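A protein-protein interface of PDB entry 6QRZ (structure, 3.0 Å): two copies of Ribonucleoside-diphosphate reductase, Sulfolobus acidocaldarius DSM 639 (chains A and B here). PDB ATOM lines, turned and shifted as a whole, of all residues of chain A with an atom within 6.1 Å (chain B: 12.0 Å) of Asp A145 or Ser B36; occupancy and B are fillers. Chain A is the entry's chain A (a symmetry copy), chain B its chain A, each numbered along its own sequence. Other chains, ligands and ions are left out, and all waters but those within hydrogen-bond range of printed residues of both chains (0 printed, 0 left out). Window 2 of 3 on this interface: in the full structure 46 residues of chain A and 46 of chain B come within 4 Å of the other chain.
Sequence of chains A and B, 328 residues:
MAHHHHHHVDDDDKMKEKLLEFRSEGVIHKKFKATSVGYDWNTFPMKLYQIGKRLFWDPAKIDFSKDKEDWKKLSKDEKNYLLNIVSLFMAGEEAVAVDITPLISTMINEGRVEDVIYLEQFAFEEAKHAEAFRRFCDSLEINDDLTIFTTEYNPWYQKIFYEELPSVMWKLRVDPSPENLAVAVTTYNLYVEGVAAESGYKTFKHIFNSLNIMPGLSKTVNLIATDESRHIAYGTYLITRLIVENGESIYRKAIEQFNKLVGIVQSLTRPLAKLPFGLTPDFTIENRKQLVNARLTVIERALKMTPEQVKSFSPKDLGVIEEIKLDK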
ATOM      1  N   ARG A 134       5.857 -10.088  14.546  1.00  0.00           N
ATOM      2  CA  ARG A 134       4.877 -11.073  14.989  1.00  0.00           C
ATOM      3  C   ARG A 134       4.327 -10.722  16.366  1.00  0.00           C
ATOM      4  O   ARG A 134       3.164 -11.019  16.664  1.00  0.00           O
ATOM      5  CB  ARG A 134       5.505 -12.467  14.999  1.00  0.00           C
ATOM      6  CG  ARG A 134       4.509 -13.610  15.123  1.00  0.00           C
ATOM      7  CD  ARG A 134       3.587 -13.685  13.917  1.00  0.00           C
ATOM      8  NE  ARG A 134       2.271 -13.116  14.189  1.00  0.00           N
ATOM      9  CZ  ARG A 134       1.276 -13.083  13.307  1.00  0.00           C
ATOM     10  NH1 ARG A 134       1.448 -13.585  12.092  1.00  0.00           N
ATOM     11  NH2 ARG A 134       0.109 -12.548  13.640  1.00  0.00           N
ATOM     12  N   ASN A 143      -4.898 -12.613  14.079  1.00  0.00           N
ATOM     13  CA  ASN A 143      -4.697 -14.051  14.180  1.00  0.00           C
ATOM     14  C   ASN A 143      -4.877 -14.778  12.855  1.00  0.00           C
ATOM     15  O   ASN A 143      -4.800 -16.011  12.829  1.00  0.00           O
ATOM     16  CB  ASN A 143      -5.649 -14.644  15.230  1.00  0.00           C
ATOM     17  CG  ASN A 143      -7.105 -14.286  14.978  1.00  0.00           C
ATOM     18  OD1 ASN A 143      -7.459 -13.762  13.923  1.00  0.00           O
ATOM     19  ND2 ASN A 143      -7.960 -14.572  15.955  1.00  0.00           N
ATOM     20  N   ASP A 144      -5.106 -14.060  11.760  1.00  0.00           N
ATOM     21  CA  ASP A 144      -5.367 -14.676  10.471  1.00  0.00           C
ATOM     22  C   ASP A 144      -4.092 -14.727   9.630  1.00  0.00           C
ATOM     23  O   ASP A 144      -3.011 -14.310  10.055  1.00  0.00           O
ATOM     24  CB  ASP A 144      -6.487 -13.933   9.740  1.00  0.00           C
ATOM     25  CG  ASP A 144      -6.219 -12.445   9.616  1.00  0.00           C
ATOM     26  OD1 ASP A 144      -5.189 -11.975  10.145  1.00  0.00           O
ATOM     27  OD2 ASP A 144      -7.040 -11.745   8.988  1.00  0.00           O
ATOM     28  N   ASP A 145      -4.232 -15.249   8.415  1.00  0.00           N
ATOM     29  CA  ASP A 145      -3.106 -15.400   7.507  1.00  0.00           C
ATOM     30  C   ASP A 145      -2.782 -14.074   6.831  1.00  0.00           C
ATOM     31  O   ASP A 145      -3.664 -13.256   6.551  1.00  0.00           O
ATOM     32  CB  ASP A 145      -3.415 -16.470   6.455  1.00  0.00           C
ATOM     33  CG  ASP A 145      -2.218 -16.796   5.572  1.00  0.00           C
ATOM     34  OD1 ASP A 145      -1.147 -16.179   5.744  1.00  0.00           O
ATOM     35  OD2 ASP A 145      -2.353 -17.681   4.700  1.00  0.00           O
ATOM     36  N   LEU A 146      -1.489 -13.870   6.570  1.00  0.00           N
ATOM     37  CA  LEU A 146      -1.001 -12.677   5.891  1.00  0.00           C
ATOM     38  C   LEU A 146      -0.299 -13.016   4.580  1.00  0.00           C
ATOM     39  O   LEU A 146       0.409 -12.171   4.026  1.00  0.00           O
ATOM     40  CB  LEU A 146      -0.066 -11.885   6.807  1.00  0.00           C
ATOM     41  CG  LEU A 146      -0.711 -11.351   8.086  1.00  0.00           C
ATOM     42  CD1 LEU A 146       0.278 -10.542   8.910  1.00  0.00           C
ATOM     43  CD2 LEU A 146      -1.944 -10.525   7.756  1.00  0.00           C
ATOM     44  N   THR A 147      -0.476 -14.241   4.078  1.00  0.00           N
ATOM     45  CA  THR A 147       0.116 -14.624   2.801  1.00  0.00           C
ATOM     46  C   THR A 147      -0.537 -13.904   1.625  1.00  0.00           C
ATOM     47  O   THR A 147       0.088 -13.772   0.567  1.00  0.00           O
ATOM     48  CB  THR A 147       0.015 -16.143   2.617  1.00  0.00           C
ATOM     49  OG1 THR A 147       0.465 -16.796   3.810  1.00  0.00           O
ATOM     50  CG2 THR A 147       0.875 -16.611   1.452  1.00  0.00           C
ATOM     51  N   ILE A 148      -1.762 -13.408   1.794  1.00  0.00           N
ATOM     52  CA  ILE A 148      -2.458 -12.691   0.730  1.00  0.00           C
ATOM     53  C   ILE A 148      -1.949 -11.256   0.653  1.00  0.00           C
ATOM     54  O   ILE A 148      -2.562 -10.402   0.003  1.00  0.00           O
ATOM     55  CB  ILE A 148      -3.984 -12.735   0.935  1.00  0.00           C
ATOM     56  CG1 ILE A 148      -4.351 -12.423   2.389  1.00  0.00           C
ATOM     57  CG2 ILE A 148      -4.539 -14.090   0.520  1.00  0.00           C
ATOM     58  CD1 ILE A 148      -4.753 -10.985   2.629  1.00  0.00           C
ATOM     59  N   PHE A 149      -0.826 -10.983   1.321  1.00  0.00           N
ATOM     60  CA  PHE A 149      -0.130  -9.710   1.212  1.00  0.00           C
ATOM     61  C   PHE A 149       1.266  -9.825   0.623  1.00  0.00           C
ATOM     62  O   PHE A 149       1.772  -8.833   0.088  1.00  0.00           O
ATOM     63  CB  PHE A 149      -0.013  -9.034   2.588  1.00  0.00           C
ATOM     64  CG  PHE A 149      -1.292  -8.421   3.077  1.00  0.00           C
ATOM     65  CD1 PHE A 149      -1.752  -7.233   2.538  1.00  0.00           C
ATOM     66  CD2 PHE A 149      -2.023  -9.022   4.087  1.00  0.00           C
ATOM     67  CE1 PHE A 149      -2.923  -6.660   2.989  1.00  0.00           C
ATOM     68  CE2 PHE A 149      -3.197  -8.454   4.544  1.00  0.00           C
ATOM     69  CZ  PHE A 149      -3.649  -7.272   3.992  1.00  0.00           C
ATOM     70  N   HIS B  29      12.039 -21.365  -0.571  1.00  0.00           N
ATOM     71  CA  HIS B  29      11.086 -20.398  -0.030  1.00  0.00           C
ATOM     72  C   HIS B  29       9.719 -20.527  -0.703  1.00  0.00           C
ATOM     73  O   HIS B  29       9.164 -19.572  -1.251  1.00  0.00           O
ATOM     74  CB  HIS B  29      11.628 -18.973  -0.147  1.00  0.00           C
ATOM     75  CG  HIS B  29      12.748 -18.679   0.801  1.00  0.00           C
ATOM     76  ND1 HIS B  29      12.542 -18.123   2.045  1.00  0.00           N
ATOM     77  CD2 HIS B  29      14.083 -18.876   0.694  1.00  0.00           C
ATOM     78  CE1 HIS B  29      13.702 -17.981   2.660  1.00  0.00           C
ATOM     79  NE2 HIS B  29      14.653 -18.433   1.863  1.00  0.00           N
ATOM     80  N   LYS B  30       9.179 -21.745  -0.648  1.00  0.00           N
ATOM     81  CA  LYS B  30       7.859 -22.002  -1.211  1.00  0.00           C
ATOM     82  C   LYS B  30       6.744 -21.466  -0.323  1.00  0.00           C
ATOM     83  O   LYS B  30       5.649 -21.175  -0.817  1.00  0.00           O
ATOM     84  CB  LYS B  30       7.674 -23.503  -1.440  1.00  0.00           C
ATOM     85  CG  LYS B  30       7.869 -24.347  -0.190  1.00  0.00           C
ATOM     86  CD  LYS B  30       7.711 -25.829  -0.488  1.00  0.00           C
ATOM     87  CE  LYS B  30       7.902 -26.668   0.765  1.00  0.00           C
ATOM     88  NZ  LYS B  30       7.744 -28.124   0.493  1.00  0.00           N
ATOM     89  N   LYS B  31       7.003 -21.318   0.974  1.00  0.00           N
ATOM     90  CA  LYS B  31       5.988 -20.869   1.915  1.00  0.00           C
ATOM     91  C   LYS B  31       6.678 -20.354   3.168  1.00  0.00           C
ATOM     92  O   LYS B  31       7.608 -20.987   3.673  1.00  0.00           O
ATOM     93  CB  LYS B  31       5.019 -22.007   2.260  1.00  0.00           C
ATOM     94  CG  LYS B  31       3.863 -21.608   3.162  1.00  0.00           C
ATOM     95  CD  LYS B  31       2.988 -22.812   3.477  1.00  0.00           C
ATOM     96  CE  LYS B  31       1.810 -22.434   4.359  1.00  0.00           C
ATOM     97  NZ  LYS B  31       0.993 -23.621   4.730  1.00  0.00           N
ATOM     98  N   PHE B  32       6.219 -19.208   3.662  1.00  0.00           N
ATOM     99  CA  PHE B  32       6.787 -18.595   4.856  1.00  0.00           C
ATOM    100  C   PHE B  32       6.020 -19.066   6.086  1.00  0.00           C
ATOM    101  O   PHE B  32       4.794 -18.929   6.149  1.00  0.00           O
ATOM    102  CB  PHE B  32       6.753 -17.071   4.752  1.00  0.00           C
ATOM    103  CG  PHE B  32       7.822 -16.499   3.865  1.00  0.00           C
ATOM    104  CD1 PHE B  32       8.895 -17.276   3.462  1.00  0.00           C
ATOM    105  CD2 PHE B  32       7.758 -15.181   3.441  1.00  0.00           C
ATOM    106  CE1 PHE B  32       9.879 -16.749   2.647  1.00  0.00           C
ATOM    107  CE2 PHE B  32       8.742 -14.650   2.628  1.00  0.00           C
ATOM    108  CZ  PHE B  32       9.804 -15.436   2.230  1.00  0.00           C
ATOM    109  N   LYS B  33       6.745 -19.612   7.065  1.00  0.00           N
ATOM    110  CA  LYS B  33       6.107 -20.071   8.293  1.00  0.00           C
ATOM    111  C   LYS B  33       5.664 -18.917   9.183  1.00  0.00           C
ATOM    112  O   LYS B  33       4.878 -19.136  10.111  1.00  0.00           O
ATOM    113  CB  LYS B  33       7.053 -20.988   9.070  1.00  0.00           C
ATOM    114  CG  LYS B  33       7.347 -22.318   8.392  1.00  0.00           C
ATOM    115  CD  LYS B  33       6.148 -23.253   8.441  1.00  0.00           C
ATOM    116  CE  LYS B  33       6.525 -24.657   7.987  1.00  0.00           C
ATOM    117  NZ  LYS B  33       7.055 -24.676   6.596  1.00  0.00           N
ATOM    118  N   ALA B  34       6.149 -17.701   8.932  1.00  0.00           N
ATOM    119  CA  ALA B  34       5.774 -16.551   9.743  1.00  0.00           C
ATOM    120  C   ALA B  34       4.559 -15.812   9.204  1.00  0.00           C
ATOM    121  O   ALA B  34       3.865 -15.140   9.976  1.00  0.00           O
ATOM    122  CB  ALA B  34       6.951 -15.577   9.857  1.00  0.00           C
ATOM    123  N   THR B  35       4.281 -15.921   7.904  1.00  0.00           N
ATOM    124  CA  THR B  35       3.132 -15.230   7.330  1.00  0.00           C
ATOM    125  C   THR B  35       1.846 -16.018   7.529  1.00  0.00           C
ATOM    126  O   THR B  35       0.804 -15.439   7.854  1.00  0.00           O
ATOM    127  CB  THR B  35       3.362 -14.973   5.841  1.00  0.00           C
ATOM    128  OG1 THR B  35       3.472 -16.223   5.150  1.00  0.00           O
ATOM    129  CG2 THR B  35       4.634 -14.181   5.636  1.00  0.00           C
ATOM    130  N   SER B  36       1.900 -17.336   7.343  1.00  0.00           N
ATOM    131  CA  SER B  36       0.699 -18.161   7.383  1.00  0.00           C
ATOM    132  C   SER B  36       0.496 -18.802   8.749  1.00  0.00           C
ATOM    133  O   SER B  36      -0.327 -18.337   9.543  1.00  0.00           O
ATOM    134  CB  SER B  36       0.766 -19.238   6.298  1.00  0.00           C
ATOM    135  OG  SER B  36       1.958 -19.993   6.411  1.00  0.00           O
ATOM    136  N   VAL B  37       1.243 -19.872   9.030  1.00  0.00           N
ATOM    137  CA  VAL B  37       1.000 -20.639  10.246  1.00  0.00           C
ATOM    138  C   VAL B  37       1.465 -19.877  11.481  1.00  0.00           C
ATOM    139  O   VAL B  37       0.959 -20.110  12.586  1.00  0.00           O
ATOM    140  CB  VAL B  37       1.670 -22.020  10.140  1.00  0.00           C
ATOM    141  CG1 VAL B  37       1.072 -22.807   8.983  1.00  0.00           C
ATOM    142  CG2 VAL B  37       3.171 -21.872   9.960  1.00  0.00           C
ATOM    143  N   GLY B  38       2.419 -18.963  11.329  1.00  0.00           N
ATOM    144  CA  GLY B  38       2.878 -18.159  12.442  1.00  0.00           C
ATOM    145  C   GLY B  38       3.900 -18.869  13.313  1.00  0.00           C
ATOM    146  O   GLY B  38       4.360 -19.977  13.036  1.00  0.00           O
ATOM    147  N   TYR B  39       4.261 -18.192  14.400  1.00  0.00           N
ATOM    148  CA  TYR B  39       5.231 -18.695  15.361  1.00  0.00           C
ATOM    149  C   TYR B  39       4.515 -19.348  16.536  1.00  0.00           C
ATOM    150  O   TYR B  39       3.521 -18.821  17.042  1.00  0.00           O
ATOM    151  CB  TYR B  39       6.134 -17.570  15.871  1.00  0.00           C
ATOM    152  CG  TYR B  39       7.106 -17.026  14.847  1.00  0.00           C
ATOM    153  CD1 TYR B  39       7.425 -17.750  13.706  1.00  0.00           C
ATOM    154  CD2 TYR B  39       7.712 -15.789  15.029  1.00  0.00           C
ATOM    155  CE1 TYR B  39       8.316 -17.255  12.771  1.00  0.00           C
ATOM    156  CE2 TYR B  39       8.604 -15.287  14.100  1.00  0.00           C
ATOM    157  CZ  TYR B  39       8.902 -16.023  12.974  1.00  0.00           C
ATOM    158  OH  TYR B  39       9.790 -15.527  12.048  1.00  0.00           O
ATOM    159  N   ASP B  40       5.032 -20.497  16.970  1.00  0.00           N
ATOM    160  CA  ASP B  40       4.510 -21.200  18.141  1.00  0.00           C
ATOM    161  C   ASP B  40       5.280 -20.714  19.364  1.00  0.00           C
ATOM    162  O   ASP B  40       6.367 -21.213  19.667  1.00  0.00           O
ATOM    163  CB  ASP B  40       4.631 -22.709  17.967  1.00  0.00           C
ATOM    164  CG  ASP B  40       3.772 -23.236  16.835  1.00  0.00           C
ATOM    165  OD1 ASP B  40       2.710 -22.639  16.562  1.00  0.00           O
ATOM    166  OD2 ASP B  40       4.162 -24.251  16.218  1.00  0.00           O
ATOM    167  N   TRP B  41       4.709 -19.738  20.073  1.00  0.00           N
ATOM    168  CA  TRP B  41       5.405 -19.128  21.200  1.00  0.00           C
ATOM    169  C   TRP B  41       5.519 -20.060  22.398  1.00  0.00           C
ATOM    170  O   TRP B  41       6.399 -19.858  23.240  1.00  0.00           O
ATOM    171  CB  TRP B  41       4.701 -17.837  21.616  1.00  0.00           C
ATOM    172  CG  TRP B  41       4.592 -16.833  20.511  1.00  0.00           C
ATOM    173  CD1 TRP B  41       3.484 -16.550  19.766  1.00  0.00           C
ATOM    174  CD2 TRP B  41       5.634 -15.984  20.020  1.00  0.00           C
ATOM    175  NE1 TRP B  41       3.772 -15.573  18.844  1.00  0.00           N
ATOM    176  CE2 TRP B  41       5.085 -15.209  18.979  1.00  0.00           C
ATOM    177  CE3 TRP B  41       6.978 -15.801  20.360  1.00  0.00           C
ATOM    178  CZ2 TRP B  41       5.832 -14.267  18.277  1.00  0.00           C
ATOM    179  CZ3 TRP B  41       7.718 -14.865  19.661  1.00  0.00           C
ATOM    180  CH2 TRP B  41       7.144 -14.111  18.632  1.00  0.00           C
ATOM    181  N   GLY B 111      12.019 -27.327   7.891  1.00  0.00           N
ATOM    182  CA  GLY B 111      10.929 -26.384   8.046  1.00  0.00           C
ATOM    183  C   GLY B 111      10.675 -25.918   9.460  1.00  0.00           C
ATOM    184  O   GLY B 111       9.694 -25.208   9.694  1.00  0.00           O
ATOM    185  N   VAL B 113      11.210 -23.516  11.611  1.00  0.00           N
ATOM    186  CA  VAL B 113      11.688 -22.141  11.730  1.00  0.00           C
ATOM    187  C   VAL B 113      11.877 -21.755  13.190  1.00  0.00           C
ATOM    188  O   VAL B 113      12.807 -21.012  13.527  1.00  0.00           O
ATOM    189  CB  VAL B 113      10.724 -21.183  11.001  1.00  0.00           C
ATOM    190  CG1 VAL B 113      11.148 -19.736  11.199  1.00  0.00           C
ATOM    191  CG2 VAL B 113      10.675 -21.523   9.522  1.00  0.00           C
ATOM    192  N   GLU B 114      11.017 -22.259  14.080  1.00  0.00           N
ATOM    193  CA  GLU B 114      11.186 -21.984  15.504  1.00  0.00           C
ATOM    194  C   GLU B 114      12.538 -22.479  15.999  1.00  0.00           C
ATOM    195  O   GLU B 114      13.218 -21.789  16.769  1.00  0.00           O
ATOM    196  CB  GLU B 114      10.054 -22.626  16.308  1.00  0.00           C
ATOM    197  CG  GLU B 114       8.658 -22.186  15.900  1.00  0.00           C
ATOM    198  CD  GLU B 114       8.114 -22.983  14.730  1.00  0.00           C
ATOM    199  OE1 GLU B 114       8.793 -23.934  14.289  1.00  0.00           O
ATOM    200  OE2 GLU B 114       7.006 -22.659  14.252  1.00  0.00           O
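OG1 of Thr A147 sits close to OG1 of Thr B35 (3.3 Å).
N of Leu A146 sits close to O of Thr B35, at 3.1 Å.
The side-chain carboxylate of Asp A145 lies close to the backbone carbonyl oxygen of Thr B35 (3.0 Å).
Among the printed residues, pairs that only touch across the chains: Arg A134 with Ala B34 (3.6 Å), Arg A134 with Tyr B39 (3.9 Å), Arg A134 with Trp B41 (3.5 Å), Asp A145 with Ser B36 (3.2 Å) and Thr A147 with Ser B36 (3.5 Å).
Asp A145 touches just these residues of chain B: Thr B35 and Ser B36.
Of chain A, only Asp A145 and Thr A147 come within 4 Å of Ser B36.
Leu A146 touches just one residue of chain B: Thr B35.
Thr A147 touches just these residues of chain B: Thr B35 (3.3 Å) and Ser B36 (3.5 Å).
No residue of chain B comes within 4 Å of Ile A148.
Of the printed residues of chain B, Arg A134 touches Ala B34, Tyr B39 and Trp B41.
Printed residues of chain A within 4 Å of Trp B41: Arg A134.
Of the printed residues of chain A, Tyr B39 touches Arg A134 (3.9 Å).
Of the printed residues of chain A, Thr B35 touches Asp A145 (3.0 Å), Leu A146 (3.1 Å) and Thr A147 (3.3 Å).
Printed residues of chain A within 4 Å of Ala B34: Arg A134 (3.6 Å).
The nearest residue of chain B that does not touch Asp A145 is Val B37 (5.5 Å).
The nearest printed residue of chain A that does not touch Tyr B39 is Asp A144 (9.3 Å).
Printed residues of chain A that touch a printed residue of chain B: Arg A134, Asp A145, Leu A146 and Thr A147.
Hydrophobic or aromatic side chains of chain A within 4 Å of the printed part of chain B: Leu A146.
Of the 16 printed residues of chain B, 5 touch a printed residue of chain A.
No position is printed for both chains.
Of the 8 pairs that touch across the chains among the printed residues, none has its exchanged pair printed and touching as well.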
